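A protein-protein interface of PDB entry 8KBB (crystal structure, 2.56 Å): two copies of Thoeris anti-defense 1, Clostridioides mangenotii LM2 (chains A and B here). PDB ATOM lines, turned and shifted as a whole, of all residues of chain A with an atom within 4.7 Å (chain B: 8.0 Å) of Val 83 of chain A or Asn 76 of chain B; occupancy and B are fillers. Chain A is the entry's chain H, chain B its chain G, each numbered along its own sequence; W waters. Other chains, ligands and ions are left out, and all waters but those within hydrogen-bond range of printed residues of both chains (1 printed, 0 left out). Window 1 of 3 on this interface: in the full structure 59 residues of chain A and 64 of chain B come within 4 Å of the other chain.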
ATOM      1  N   LEU A  79      -9.844 -10.272  25.986  1.00  0.00           N
ATOM      2  CA  LEU A  79      -8.441  -9.940  26.211  1.00  0.00           C
ATOM      3  C   LEU A  79      -8.275  -9.033  27.423  1.00  0.00           C
ATOM      4  O   LEU A  79      -7.377  -9.242  28.250  1.00  0.00           O
ATOM      5  CB  LEU A  79      -7.856  -9.283  24.968  1.00  0.00           C
ATOM      6  CG  LEU A  79      -8.090 -10.036  23.669  1.00  0.00           C
ATOM      7  CD1 LEU A  79      -7.269  -9.390  22.580  1.00  0.00           C
ATOM      8  CD2 LEU A  79      -7.711 -11.503  23.833  1.00  0.00           C
ATOM      9  N   ILE A  80      -9.133  -8.024  27.545  1.00  0.00           N
ATOM     10  CA  ILE A  80      -9.055  -7.164  28.717  1.00  0.00           C
ATOM     11  C   ILE A  80      -9.288  -7.975  29.979  1.00  0.00           C
ATOM     12  O   ILE A  80      -8.661  -7.724  31.015  1.00  0.00           O
ATOM     13  CB  ILE A  80     -10.050  -5.991  28.598  1.00  0.00           C
ATOM     14  CG1 ILE A  80      -9.629  -5.062  27.460  1.00  0.00           C
ATOM     15  CG2 ILE A  80     -10.140  -5.229  29.912  1.00  0.00           C
ATOM     16  CD1 ILE A  80     -10.807  -4.435  26.754  1.00  0.00           C
ATOM     17  N   LEU A  81     -10.174  -8.966  29.917  1.00  0.00           N
ATOM     18  CA  LEU A  81     -10.444  -9.777  31.091  1.00  0.00           C
ATOM     19  C   LEU A  81      -9.207 -10.564  31.502  1.00  0.00           C
ATOM     20  O   LEU A  81      -8.880 -10.628  32.694  1.00  0.00           O
ATOM     21  CB  LEU A  81     -11.631 -10.699  30.813  1.00  0.00           C
ATOM     22  CG  LEU A  81     -11.976 -11.692  31.914  1.00  0.00           C
ATOM     23  CD1 LEU A  81     -12.364 -10.909  33.142  1.00  0.00           C
ATOM     24  CD2 LEU A  81     -13.104 -12.607  31.470  1.00  0.00           C
ATOM     25  N   MET A  82      -8.444 -11.083  30.578  1.00  0.00           N
ATOM     26  CA  MET A  82      -7.235 -11.777  30.897  1.00  0.00           C
ATOM     27  C   MET A  82      -6.190 -10.911  31.560  1.00  0.00           C
ATOM     28  O   MET A  82      -5.492 -11.364  32.432  1.00  0.00           O
ATOM     29  CB  MET A  82      -6.723 -12.449  29.639  1.00  0.00           C
ATOM     30  CG  MET A  82      -7.719 -13.404  29.026  1.00  0.00           C
ATOM     31  SD  MET A  82      -7.476 -13.783  27.292  1.00  0.00           S
ATOM     32  CE  MET A  82      -5.742 -13.685  27.247  1.00  0.00           C
ATOM     33  N   VAL A  83      -6.052  -9.676  31.123  1.00  0.00           N
ATOM     34  CA  VAL A  83      -5.101  -8.750  31.694  1.00  0.00           C
ATOM     35  C   VAL A  83      -5.467  -8.330  33.107  1.00  0.00           C
ATOM     36  O   VAL A  83      -4.632  -8.276  33.962  1.00  0.00           O
ATOM     37  CB  VAL A  83      -4.798  -7.580  30.720  1.00  0.00           C
ATOM     38  CG1 VAL A  83      -3.823  -6.589  31.302  1.00  0.00           C
ATOM     39  CG2 VAL A  83      -4.339  -8.092  29.373  1.00  0.00           C
ATOM     40  N   ILE A  84      -6.726  -8.086  33.362  1.00  0.00           N
ATOM     41  CA  ILE A  84      -7.141  -7.741  34.683  1.00  0.00           C
ATOM     42  C   ILE A  84      -6.840  -8.867  35.608  1.00  0.00           C
ATOM     43  O   ILE A  84      -6.331  -8.655  36.662  1.00  0.00           O
ATOM     44  CB  ILE A  84      -8.639  -7.371  34.728  1.00  0.00           C
ATOM     45  CG1 ILE A  84      -8.909  -6.148  33.875  1.00  0.00           C
ATOM     46  CG2 ILE A  84      -9.116  -7.095  36.137  1.00  0.00           C
ATOM     47  CD1 ILE A  84     -10.364  -5.778  33.782  1.00  0.00           C
ATOM     48  N   THR A  85      -7.089 -10.071  35.175  1.00  0.00           N
ATOM     49  CA  THR A  85      -6.856 -11.230  35.989  1.00  0.00           C
ATOM     50  C   THR A  85      -5.389 -11.394  36.354  1.00  0.00           C
ATOM     51  O   THR A  85      -5.051 -11.589  37.490  1.00  0.00           O
ATOM     52  CB  THR A  85      -7.434 -12.454  35.243  1.00  0.00           C
ATOM     53  OG1 THR A  85      -8.829 -12.263  35.041  1.00  0.00           O
ATOM     54  CG2 THR A  85      -7.216 -13.731  35.987  1.00  0.00           C
ATOM     55  N   ARG A  86      -4.518 -11.225  35.402  1.00  0.00           N
ATOM     56  CA  ARG A  86      -3.126 -11.320  35.658  1.00  0.00           C
ATOM     57  C   ARG A  86      -2.581 -10.252  36.537  1.00  0.00           C
ATOM     58  O   ARG A  86      -1.728 -10.498  37.325  1.00  0.00           O
ATOM     59  CB  ARG A  86      -2.400 -11.370  34.328  1.00  0.00           C
ATOM     60  CG  ARG A  86      -2.532 -12.705  33.667  1.00  0.00           C
ATOM     61  CD  ARG A  86      -1.875 -12.717  32.319  1.00  0.00           C
ATOM     62  NE  ARG A  86      -0.658 -11.927  32.242  1.00  0.00           N
ATOM     63  CZ  ARG A  86       0.554 -12.353  32.562  1.00  0.00           C
ATOM     64  NH1 ARG A  86       0.741 -13.573  33.009  1.00  0.00           N
ATOM     65  NH2 ARG A  86       1.580 -11.548  32.433  1.00  0.00           N
ATOM     66  N   LEU A  87      -3.037  -9.040  36.349  1.00  0.00           N
ATOM     67  CA  LEU A  87      -2.605  -7.950  37.139  1.00  0.00           C
ATOM     68  C   LEU A  87      -3.049  -8.082  38.544  1.00  0.00           C
ATOM     69  O   LEU A  87      -2.323  -7.774  39.443  1.00  0.00           O
ATOM     70  CB  LEU A  87      -3.044  -6.650  36.505  1.00  0.00           C
ATOM     71  CG  LEU A  87      -2.355  -6.122  35.271  1.00  0.00           C
ATOM     72  CD1 LEU A  87      -3.075  -4.859  34.844  1.00  0.00           C
ATOM     73  CD2 LEU A  87      -0.906  -5.848  35.601  1.00  0.00           C
ATOM     74  N   PHE A  90      -0.796 -10.372  40.312  1.00  0.00           N
ATOM     75  CA  PHE A  90       0.421  -9.750  40.726  1.00  0.00           C
ATOM     76  C   PHE A  90       0.236  -8.881  41.945  1.00  0.00           C
ATOM     77  O   PHE A  90       1.164  -8.578  42.620  1.00  0.00           O
ATOM     78  CB  PHE A  90       1.012  -8.924  39.605  1.00  0.00           C
ATOM     79  CG  PHE A  90       1.334  -9.679  38.362  1.00  0.00           C
ATOM     80  CD1 PHE A  90       1.894 -10.931  38.408  1.00  0.00           C
ATOM     81  CD2 PHE A  90       1.141  -9.085  37.133  1.00  0.00           C
ATOM     82  CE1 PHE A  90       2.213 -11.595  37.248  1.00  0.00           C
ATOM     83  CE2 PHE A  90       1.446  -9.750  35.967  1.00  0.00           C
ATOM     84  CZ  PHE A  90       1.980 -11.010  36.028  1.00  0.00           C
ATOM     85  N   LEU A 107      -8.644  -0.486  33.256  1.00  0.00           N
ATOM     86  CA  LEU A 107      -9.195  -1.570  32.443  1.00  0.00           C
ATOM     87  C   LEU A 107     -10.643  -1.856  32.811  1.00  0.00           C
ATOM     88  O   LEU A 107     -11.479  -2.110  31.932  1.00  0.00           O
ATOM     89  CB  LEU A 107      -8.347  -2.826  32.598  1.00  0.00           C
ATOM     90  CG  LEU A 107      -6.957  -2.703  31.980  1.00  0.00           C
ATOM     91  CD1 LEU A 107      -6.098  -3.901  32.335  1.00  0.00           C
ATOM     92  CD2 LEU A 107      -7.073  -2.550  30.476  1.00  0.00           C
ATOM     93  N   ILE B  13     -12.891 -17.966  34.122  1.00  0.00           N
ATOM     94  CA  ILE B  13     -12.637 -16.609  34.579  1.00  0.00           C
ATOM     95  C   ILE B  13     -13.919 -15.818  34.436  1.00  0.00           C
ATOM     96  O   ILE B  13     -14.438 -15.651  33.333  1.00  0.00           O
ATOM     97  CB  ILE B  13     -11.499 -15.947  33.803  1.00  0.00           C
ATOM     98  CG1 ILE B  13     -10.262 -16.834  33.878  1.00  0.00           C
ATOM     99  CG2 ILE B  13     -11.219 -14.570  34.374  1.00  0.00           C
ATOM    100  CD1 ILE B  13      -9.605 -16.816  35.253  1.00  0.00           C
ATOM    101  N   VAL B  25     -14.014 -17.610  29.079  1.00  0.00           N
ATOM    102  CA  VAL B  25     -12.596 -17.462  29.270  1.00  0.00           C
ATOM    103  C   VAL B  25     -12.137 -18.387  30.343  1.00  0.00           C
ATOM    104  O   VAL B  25     -12.748 -18.503  31.361  1.00  0.00           O
ATOM    105  CB  VAL B  25     -12.216 -15.995  29.552  1.00  0.00           C
ATOM    106  CG1 VAL B  25     -10.758 -15.851  29.939  1.00  0.00           C
ATOM    107  CG2 VAL B  25     -12.509 -15.130  28.344  1.00  0.00           C
ATOM    108  N   ALA B  37       0.883 -15.800  38.403  1.00  0.00           N
ATOM    109  CA  ALA B  37      -0.273 -15.423  37.596  1.00  0.00           C
ATOM    110  C   ALA B  37      -0.648 -16.596  36.666  1.00  0.00           C
ATOM    111  O   ALA B  37       0.146 -17.485  36.457  1.00  0.00           O
ATOM    112  CB  ALA B  37       0.009 -14.177  36.753  1.00  0.00           C
ATOM    113  N   PRO B  38      -1.877 -16.558  36.151  1.00  0.00           N
ATOM    114  CA  PRO B  38      -2.181 -17.466  35.026  1.00  0.00           C
ATOM    115  C   PRO B  38      -1.449 -17.004  33.778  1.00  0.00           C
ATOM    116  O   PRO B  38      -1.243 -15.807  33.571  1.00  0.00           O
ATOM    117  CB  PRO B  38      -3.702 -17.332  34.873  1.00  0.00           C
ATOM    118  CG  PRO B  38      -4.035 -15.998  35.492  1.00  0.00           C
ATOM    119  CD  PRO B  38      -3.037 -15.778  36.582  1.00  0.00           C
ATOM    120  N   PHE B  41      -4.432 -19.063  28.838  1.00  0.00           N
ATOM    121  CA  PHE B  41      -5.855 -18.807  28.736  1.00  0.00           C
ATOM    122  C   PHE B  41      -6.411 -19.479  27.493  1.00  0.00           C
ATOM    123  O   PHE B  41      -5.689 -19.812  26.547  1.00  0.00           O
ATOM    124  CB  PHE B  41      -6.137 -17.304  28.678  1.00  0.00           C
ATOM    125  CG  PHE B  41      -5.938 -16.594  29.985  1.00  0.00           C
ATOM    126  CD1 PHE B  41      -4.663 -16.243  30.409  1.00  0.00           C
ATOM    127  CD2 PHE B  41      -7.022 -16.258  30.780  1.00  0.00           C
ATOM    128  CE1 PHE B  41      -4.467 -15.578  31.605  1.00  0.00           C
ATOM    129  CE2 PHE B  41      -6.838 -15.584  31.979  1.00  0.00           C
ATOM    130  CZ  PHE B  41      -5.549 -15.243  32.392  1.00  0.00           C
ATOM    131  N   PHE B  61       0.768 -16.281  27.754  1.00  0.00           N
ATOM    132  CA  PHE B  61       1.562 -15.126  28.137  1.00  0.00           C
ATOM    133  C   PHE B  61       2.982 -15.537  28.469  1.00  0.00           C
ATOM    134  O   PHE B  61       3.237 -16.663  28.895  1.00  0.00           O
ATOM    135  CB  PHE B  61       0.974 -14.410  29.349  1.00  0.00           C
ATOM    136  CG  PHE B  61      -0.348 -13.780  29.098  1.00  0.00           C
ATOM    137  CD1 PHE B  61      -1.501 -14.528  29.177  1.00  0.00           C
ATOM    138  CD2 PHE B  61      -0.438 -12.429  28.796  1.00  0.00           C
ATOM    139  CE1 PHE B  61      -2.719 -13.946  28.961  1.00  0.00           C
ATOM    140  CE2 PHE B  61      -1.660 -11.835  28.574  1.00  0.00           C
ATOM    141  CZ  PHE B  61      -2.804 -12.591  28.653  1.00  0.00           C
ATOM    142  N   GLN B  62       3.892 -14.591  28.286  1.00  0.00           N
ATOM    143  CA  GLN B  62       5.268 -14.708  28.736  1.00  0.00           C
ATOM    144  C   GLN B  62       5.334 -15.219  30.173  1.00  0.00           C
ATOM    145  O   GLN B  62       4.766 -14.607  31.083  1.00  0.00           O
ATOM    146  CB  GLN B  62       5.932 -13.339  28.622  1.00  0.00           C
ATOM    147  CG  GLN B  62       7.287 -13.272  29.248  1.00  0.00           C
ATOM    148  CD  GLN B  62       8.287 -14.121  28.503  1.00  0.00           C
ATOM    149  OE1 GLN B  62       8.221 -14.245  27.280  1.00  0.00           O
ATOM    150  NE2 GLN B  62       9.218 -14.722  29.237  1.00  0.00           N
ATOM    151  N   GLY B  73       5.888 -16.004  25.013  1.00  0.00           N
ATOM    152  CA  GLY B  73       4.485 -15.674  25.154  1.00  0.00           C
ATOM    153  C   GLY B  73       4.283 -14.187  24.974  1.00  0.00           C
ATOM    154  O   GLY B  73       5.240 -13.418  24.814  1.00  0.00           O
ATOM    155  N   VAL B  74       3.012 -13.787  24.993  1.00  0.00           N
ATOM    156  CA  VAL B  74       2.659 -12.387  24.785  1.00  0.00           C
ATOM    157  C   VAL B  74       2.643 -11.664  26.121  1.00  0.00           C
ATOM    158  O   VAL B  74       2.585 -12.274  27.190  1.00  0.00           O
ATOM    159  CB  VAL B  74       1.302 -12.219  24.075  1.00  0.00           C
ATOM    160  CG1 VAL B  74       1.307 -12.972  22.766  1.00  0.00           C
ATOM    161  CG2 VAL B  74       0.153 -12.661  24.992  1.00  0.00           C
ATOM    162  N   ASN B  75       2.661 -10.340  26.045  1.00  0.00           N
ATOM    163  CA  ASN B  75       2.557  -9.460  27.196  1.00  0.00           C
ATOM    164  C   ASN B  75       1.201  -8.766  27.209  1.00  0.00           C
ATOM    165  O   ASN B  75       0.540  -8.627  26.177  1.00  0.00           O
ATOM    166  CB  ASN B  75       3.687  -8.434  27.169  1.00  0.00           C
ATOM    167  CG  ASN B  75       5.050  -9.097  27.177  1.00  0.00           C
ATOM    168  OD1 ASN B  75       5.384  -9.816  28.120  1.00  0.00           O
ATOM    169  ND2 ASN B  75       5.827  -8.900  26.111  1.00  0.00           N
ATOM    170  N   ASN B  76       0.786  -8.357  28.408  1.00  0.00           N
ATOM    171  CA  ASN B  76      -0.436  -7.576  28.571  1.00  0.00           C
ATOM    172  C   ASN B  76      -0.507  -6.466  27.537  1.00  0.00           C
ATOM    173  O   ASN B  76      -1.541  -6.247  26.884  1.00  0.00           O
ATOM    174  CB  ASN B  76      -0.469  -6.978  29.980  1.00  0.00           C
ATOM    175  CG  ASN B  76      -0.598  -8.023  31.046  1.00  0.00           C
ATOM    176  OD1 ASN B  76      -1.023  -9.147  30.776  1.00  0.00           O
ATOM    177  ND2 ASN B  76      -0.211  -7.674  32.266  1.00  0.00           N
ATOM    178  N   GLU B  77       0.613  -5.766  27.381  1.00  0.00           N
ATOM    179  CA  GLU B  77       0.677  -4.605  26.510  1.00  0.00           C
ATOM    180  C   GLU B  77       0.292  -4.958  25.075  1.00  0.00           C
ATOM    181  O   GLU B  77      -0.374  -4.165  24.396  1.00  0.00           O
ATOM    182  CB  GLU B  77       2.079  -4.001  26.590  1.00  0.00           C
ATOM    183  CG  GLU B  77       2.368  -3.364  27.947  1.00  0.00           C
ATOM    184  CD  GLU B  77       2.986  -4.327  28.975  1.00  0.00           C
ATOM    185  OE1 GLU B  77       3.800  -3.868  29.811  1.00  0.00           O
ATOM    186  OE2 GLU B  77       2.652  -5.537  28.959  1.00  0.00           O
ATOM    187  N   ASP B  78       0.664  -6.156  24.608  1.00  0.00           N
ATOM    188  CA  ASP B  78       0.353  -6.546  23.233  1.00  0.00           C
ATOM    189  C   ASP B  78      -1.152  -6.674  23.032  1.00  0.00           C
ATOM    190  O   ASP B  78      -1.712  -6.171  22.043  1.00  0.00           O
ATOM    191  CB  ASP B  78       1.055  -7.862  22.885  1.00  0.00           C
ATOM    192  CG  ASP B  78       2.562  -7.791  23.078  1.00  0.00           C
ATOM    193  OD1 ASP B  78       3.163  -6.752  22.741  1.00  0.00           O
ATOM    194  OD2 ASP B  78       3.150  -8.773  23.571  1.00  0.00           O
ATOM    195  N   LEU B  79      -1.824  -7.341  23.973  1.00  0.00           N
ATOM    196  CA  LEU B  79      -3.268  -7.511  23.876  1.00  0.00           C
ATOM    197  C   LEU B  79      -3.973  -6.164  23.925  1.00  0.00           C
ATOM    198  O   LEU B  79      -4.887  -5.883  23.126  1.00  0.00           O
ATOM    199  CB  LEU B  79      -3.753  -8.421  25.005  1.00  0.00           C
ATOM    200  CG  LEU B  79      -3.090  -9.803  25.117  1.00  0.00           C
ATOM    201  CD1 LEU B  79      -3.924 -10.693  26.017  1.00  0.00           C
ATOM    202  CD2 LEU B  79      -2.848 -10.486  23.748  1.00  0.00           C
ATOM    203  N   ILE B  80      -3.554  -5.310  24.861  1.00  0.00           N
ATOM    204  CA  ILE B  80      -4.178  -3.998  24.975  1.00  0.00           C
ATOM    205  C   ILE B  80      -3.991  -3.210  23.689  1.00  0.00           C
ATOM    206  O   ILE B  80      -4.890  -2.481  23.255  1.00  0.00           O
ATOM    207  CB  ILE B  80      -3.613  -3.246  26.187  1.00  0.00           C
ATOM    208  CG1 ILE B  80      -3.975  -3.979  27.475  1.00  0.00           C
ATOM    209  CG2 ILE B  80      -4.130  -1.815  26.211  1.00  0.00           C
ATOM    210  CD1 ILE B  80      -3.242  -3.411  28.692  1.00  0.00           C
ATOM    211  N   LEU B  81      -2.828  -3.351  23.052  1.00  0.00           N
ATOM    212  CA  LEU B  81      -2.594  -2.627  21.806  1.00  0.00           C
ATOM    213  C   LEU B  81      -3.508  -3.135  20.699  1.00  0.00           C
ATOM    214  O   LEU B  81      -4.013  -2.342  19.895  1.00  0.00           O
ATOM    215  CB  LEU B  81      -1.131  -2.742  21.394  1.00  0.00           C
ATOM    216  CG  LEU B  81      -0.771  -2.112  20.052  1.00  0.00           C
ATOM    217  CD1 LEU B  81      -1.280  -0.678  19.971  1.00  0.00           C
ATOM    218  CD2 LEU B  81       0.739  -2.172  19.832  1.00  0.00           C
ATOM    219  N   MET B  82      -3.729  -4.448  20.634  1.00  0.00           N
ATOM    220  CA  MET B  82      -4.728  -4.968  19.698  1.00  0.00           C
ATOM    221  C   MET B  82      -6.087  -4.319  19.920  1.00  0.00           C
ATOM    222  O   MET B  82      -6.761  -3.897  18.962  1.00  0.00           O
ATOM    223  CB  MET B  82      -4.846  -6.475  19.846  1.00  0.00           C
ATOM    224  CG  MET B  82      -3.563  -7.187  19.607  1.00  0.00           C
ATOM    225  SD  MET B  82      -3.896  -8.917  19.725  1.00  0.00           S
ATOM    226  CE  MET B  82      -2.207  -9.483  19.806  1.00  0.00           C
ATOM    227  N   VAL B  83      -6.516  -4.248  21.181  1.00  0.00           N
ATOM    228  CA  VAL B  83      -7.850  -3.713  21.441  1.00  0.00           C
ATOM    229  C   VAL B  83      -7.902  -2.238  21.083  1.00  0.00           C
ATOM    230  O   VAL B  83      -8.895  -1.754  20.530  1.00  0.00           O
ATOM    231  CB  VAL B  83      -8.273  -3.962  22.896  1.00  0.00           C
ATOM    232  CG1 VAL B  83      -9.625  -3.343  23.148  1.00  0.00           C
ATOM    233  CG2 VAL B  83      -8.306  -5.457  23.179  1.00  0.00           C
ATOM    234  N   LEU B 107      -7.727   2.620  27.880  1.00  0.00           N
ATOM    235  CA  LEU B 107      -6.687   1.661  27.516  1.00  0.00           C
ATOM    236  C   LEU B 107      -5.335   2.338  27.341  1.00  0.00           C
ATOM    237  O   LEU B 107      -4.300   1.801  27.760  1.00  0.00           O
ATOM    238  CB  LEU B 107      -7.078   0.922  26.244  1.00  0.00           C
ATOM    239  CG  LEU B 107      -8.307   0.037  26.375  1.00  0.00           C
ATOM    240  CD1 LEU B 107      -8.761  -0.391  25.002  1.00  0.00           C
ATOM    241  CD2 LEU B 107      -8.013  -1.168  27.248  1.00  0.00           C
ATOM    242  N   CYS B 110      -4.069   2.988  30.735  1.00  0.00           N
ATOM    243  CA  CYS B 110      -3.562   1.740  31.290  1.00  0.00           C
ATOM    244  C   CYS B 110      -2.152   1.468  30.784  1.00  0.00           C
ATOM    245  O   CYS B 110      -1.250   1.117  31.563  1.00  0.00           O
ATOM    246  CB  CYS B 110      -4.507   0.597  30.931  1.00  0.00           C
ATOM    247  SG  CYS B 110      -3.875  -1.051  31.292  1.00  0.00           S
ATOM    248  N   LEU B 111      -1.945   1.637  29.471  1.00  0.00           N
ATOM    249  CA  LEU B 111      -0.612   1.452  28.903  1.00  0.00           C
ATOM    250  C   LEU B 111       0.383   2.439  29.509  1.00  0.00           C
ATOM    251  O   LEU B 111       1.544   2.091  29.742  1.00  0.00           O
ATOM    252  CB  LEU B 111      -0.654   1.578  27.376  1.00  0.00           C
ATOM    253  CG  LEU B 111      -1.205   0.347  26.635  1.00  0.00           C
ATOM    254  CD1 LEU B 111      -1.013   0.436  25.140  1.00  0.00           C
ATOM    255  CD2 LEU B 111      -0.610  -0.951  27.154  1.00  0.00           C
ATOM    256  N   LEU B 114       1.242   1.112  33.203  1.00  0.00           N
ATOM    257  CA  LEU B 114       2.175  -0.005  33.074  1.00  0.00           C
ATOM    258  C   LEU B 114       3.526   0.467  32.555  1.00  0.00           C
ATOM    259  O   LEU B 114       4.577  -0.055  32.954  1.00  0.00           O
ATOM    260  CB  LEU B 114       1.590  -1.076  32.148  1.00  0.00           C
ATOM    261  CG  LEU B 114       0.292  -1.758  32.604  1.00  0.00           C
ATOM    262  CD1 LEU B 114      -0.158  -2.744  31.558  1.00  0.00           C
ATOM    263  CD2 LEU B 114       0.458  -2.453  33.964  1.00  0.00           C
HETATM  264  O   HOH W   1       2.765  -8.986  30.834  1.00  0.00           O
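The backbone carbonyl oxygen of Pro 38 of chain B sits at hydrogen-bond distance from the guanidinium group of Arg 86 of chain A, at 3.0 Å. The guanidinium group of Arg 86 of chain A is in hydrogen-bond range of the side-chain amide oxygen of Asn 76 of chain B, at 3.2 Å.
The backbone NH of Ile 13 of chain B lies within hydrogen-bond range of the backbone carbonyl oxygen of Val 25 of chain B (2.8 Å). The side-chain hydroxyl of Thr 85 of chain A lies within hydrogen-bond range of the backbone carbonyl oxygen of Leu 81 of chain A (2.9 Å).
Leu 81 of chain A touches Ile 13 of chain B. CB of Val 25 of chain B touches CD2 of Leu 81 of chain A (3.99 Å). Met 82 of chain A touches Phe 61 of chain B (CE to CZ, 3.4 Å). CG1 of Val 83 of chain A touches CG of Asn 76 of chain B, 3.5 Å away. CG2 of Thr 85 of chain A touches CG of Pro 38 of chain B, at 3.9 Å. Arg 86 of chain A touches Ala 37 of chain B (NH1 to CB, 3.9 Å). Arg 86 of chain A touches Phe 41 of chain B (CD to CE1, 3.9 Å). CD2 of Leu 87 of chain A touches ND2 of Asn 76 of chain B (3.9 Å). CD2 of Leu 107 of chain A touches CD2 of Leu 107 of chain B, 3.6 Å away. SG of Cys 110 of chain B touches CG of Leu 107 of chain A (3.6 Å).
Printed residues of chain A within 4 Å of Asn 76 of chain B: Val 83 (3.5 Å), Arg 86 (3.2 Å) and Leu 87 (3.9 Å). Of the printed residues of chain B, Leu 107 of chain A touches Leu 107 (3.6 Å) and Cys 110 (3.6 Å). Printed residues of chain A within 4 Å of Leu 79 of chain B: Met 82. Printed residues of chain A within 4 Å of Val 83 of chain B: Ile 80 (3.9 Å). Gln 62 of chain B touches none of the printed residues of chain A. The nearest residue of chain B that does not touch Val 83 of chain A is Ile 80 of chain B (4.2 Å). The nearest residue of chain A that does not touch Asn 76 of chain B is Phe 90 of chain A (4.6 Å).
Of the 11 printed residues of chain A, 9 touch a printed residue of chain B. Hydrophobic or aromatic side chains of chain A within 4 Å of the printed part of chain B: Ile 80, Leu 81, Met 82, Val 83, Leu 87, Phe 90 and Leu 107. Along chain A the printed residues that touch a printed residue of chain B span positions 80 to 107. Among the printed residues, 18 pairs touch across the chains.
Ile 80 of chain A touches Val 83 of chain B, but with the chains exchanged Val 83 of chain A does not touch Ile 80 of chain B (4.2 Å). Met 82 of chain A touches Leu 79 of chain B, but with the chains exchanged Leu 79 of chain A does not touch Met 82 of chain B (4.4 Å). Leu 107 of chain A touches its own counterpart, Leu 107 of chain B. Of the 18 pairs that touch across the chains among the printed residues, 1 has its exchanged pair printed and touching as well.
Water W1 lies within hydrogen-bond range of the backbone NH (N) of Asn 76 of chain B and the guanidinium group (NH2) of Arg 86 of chain A.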
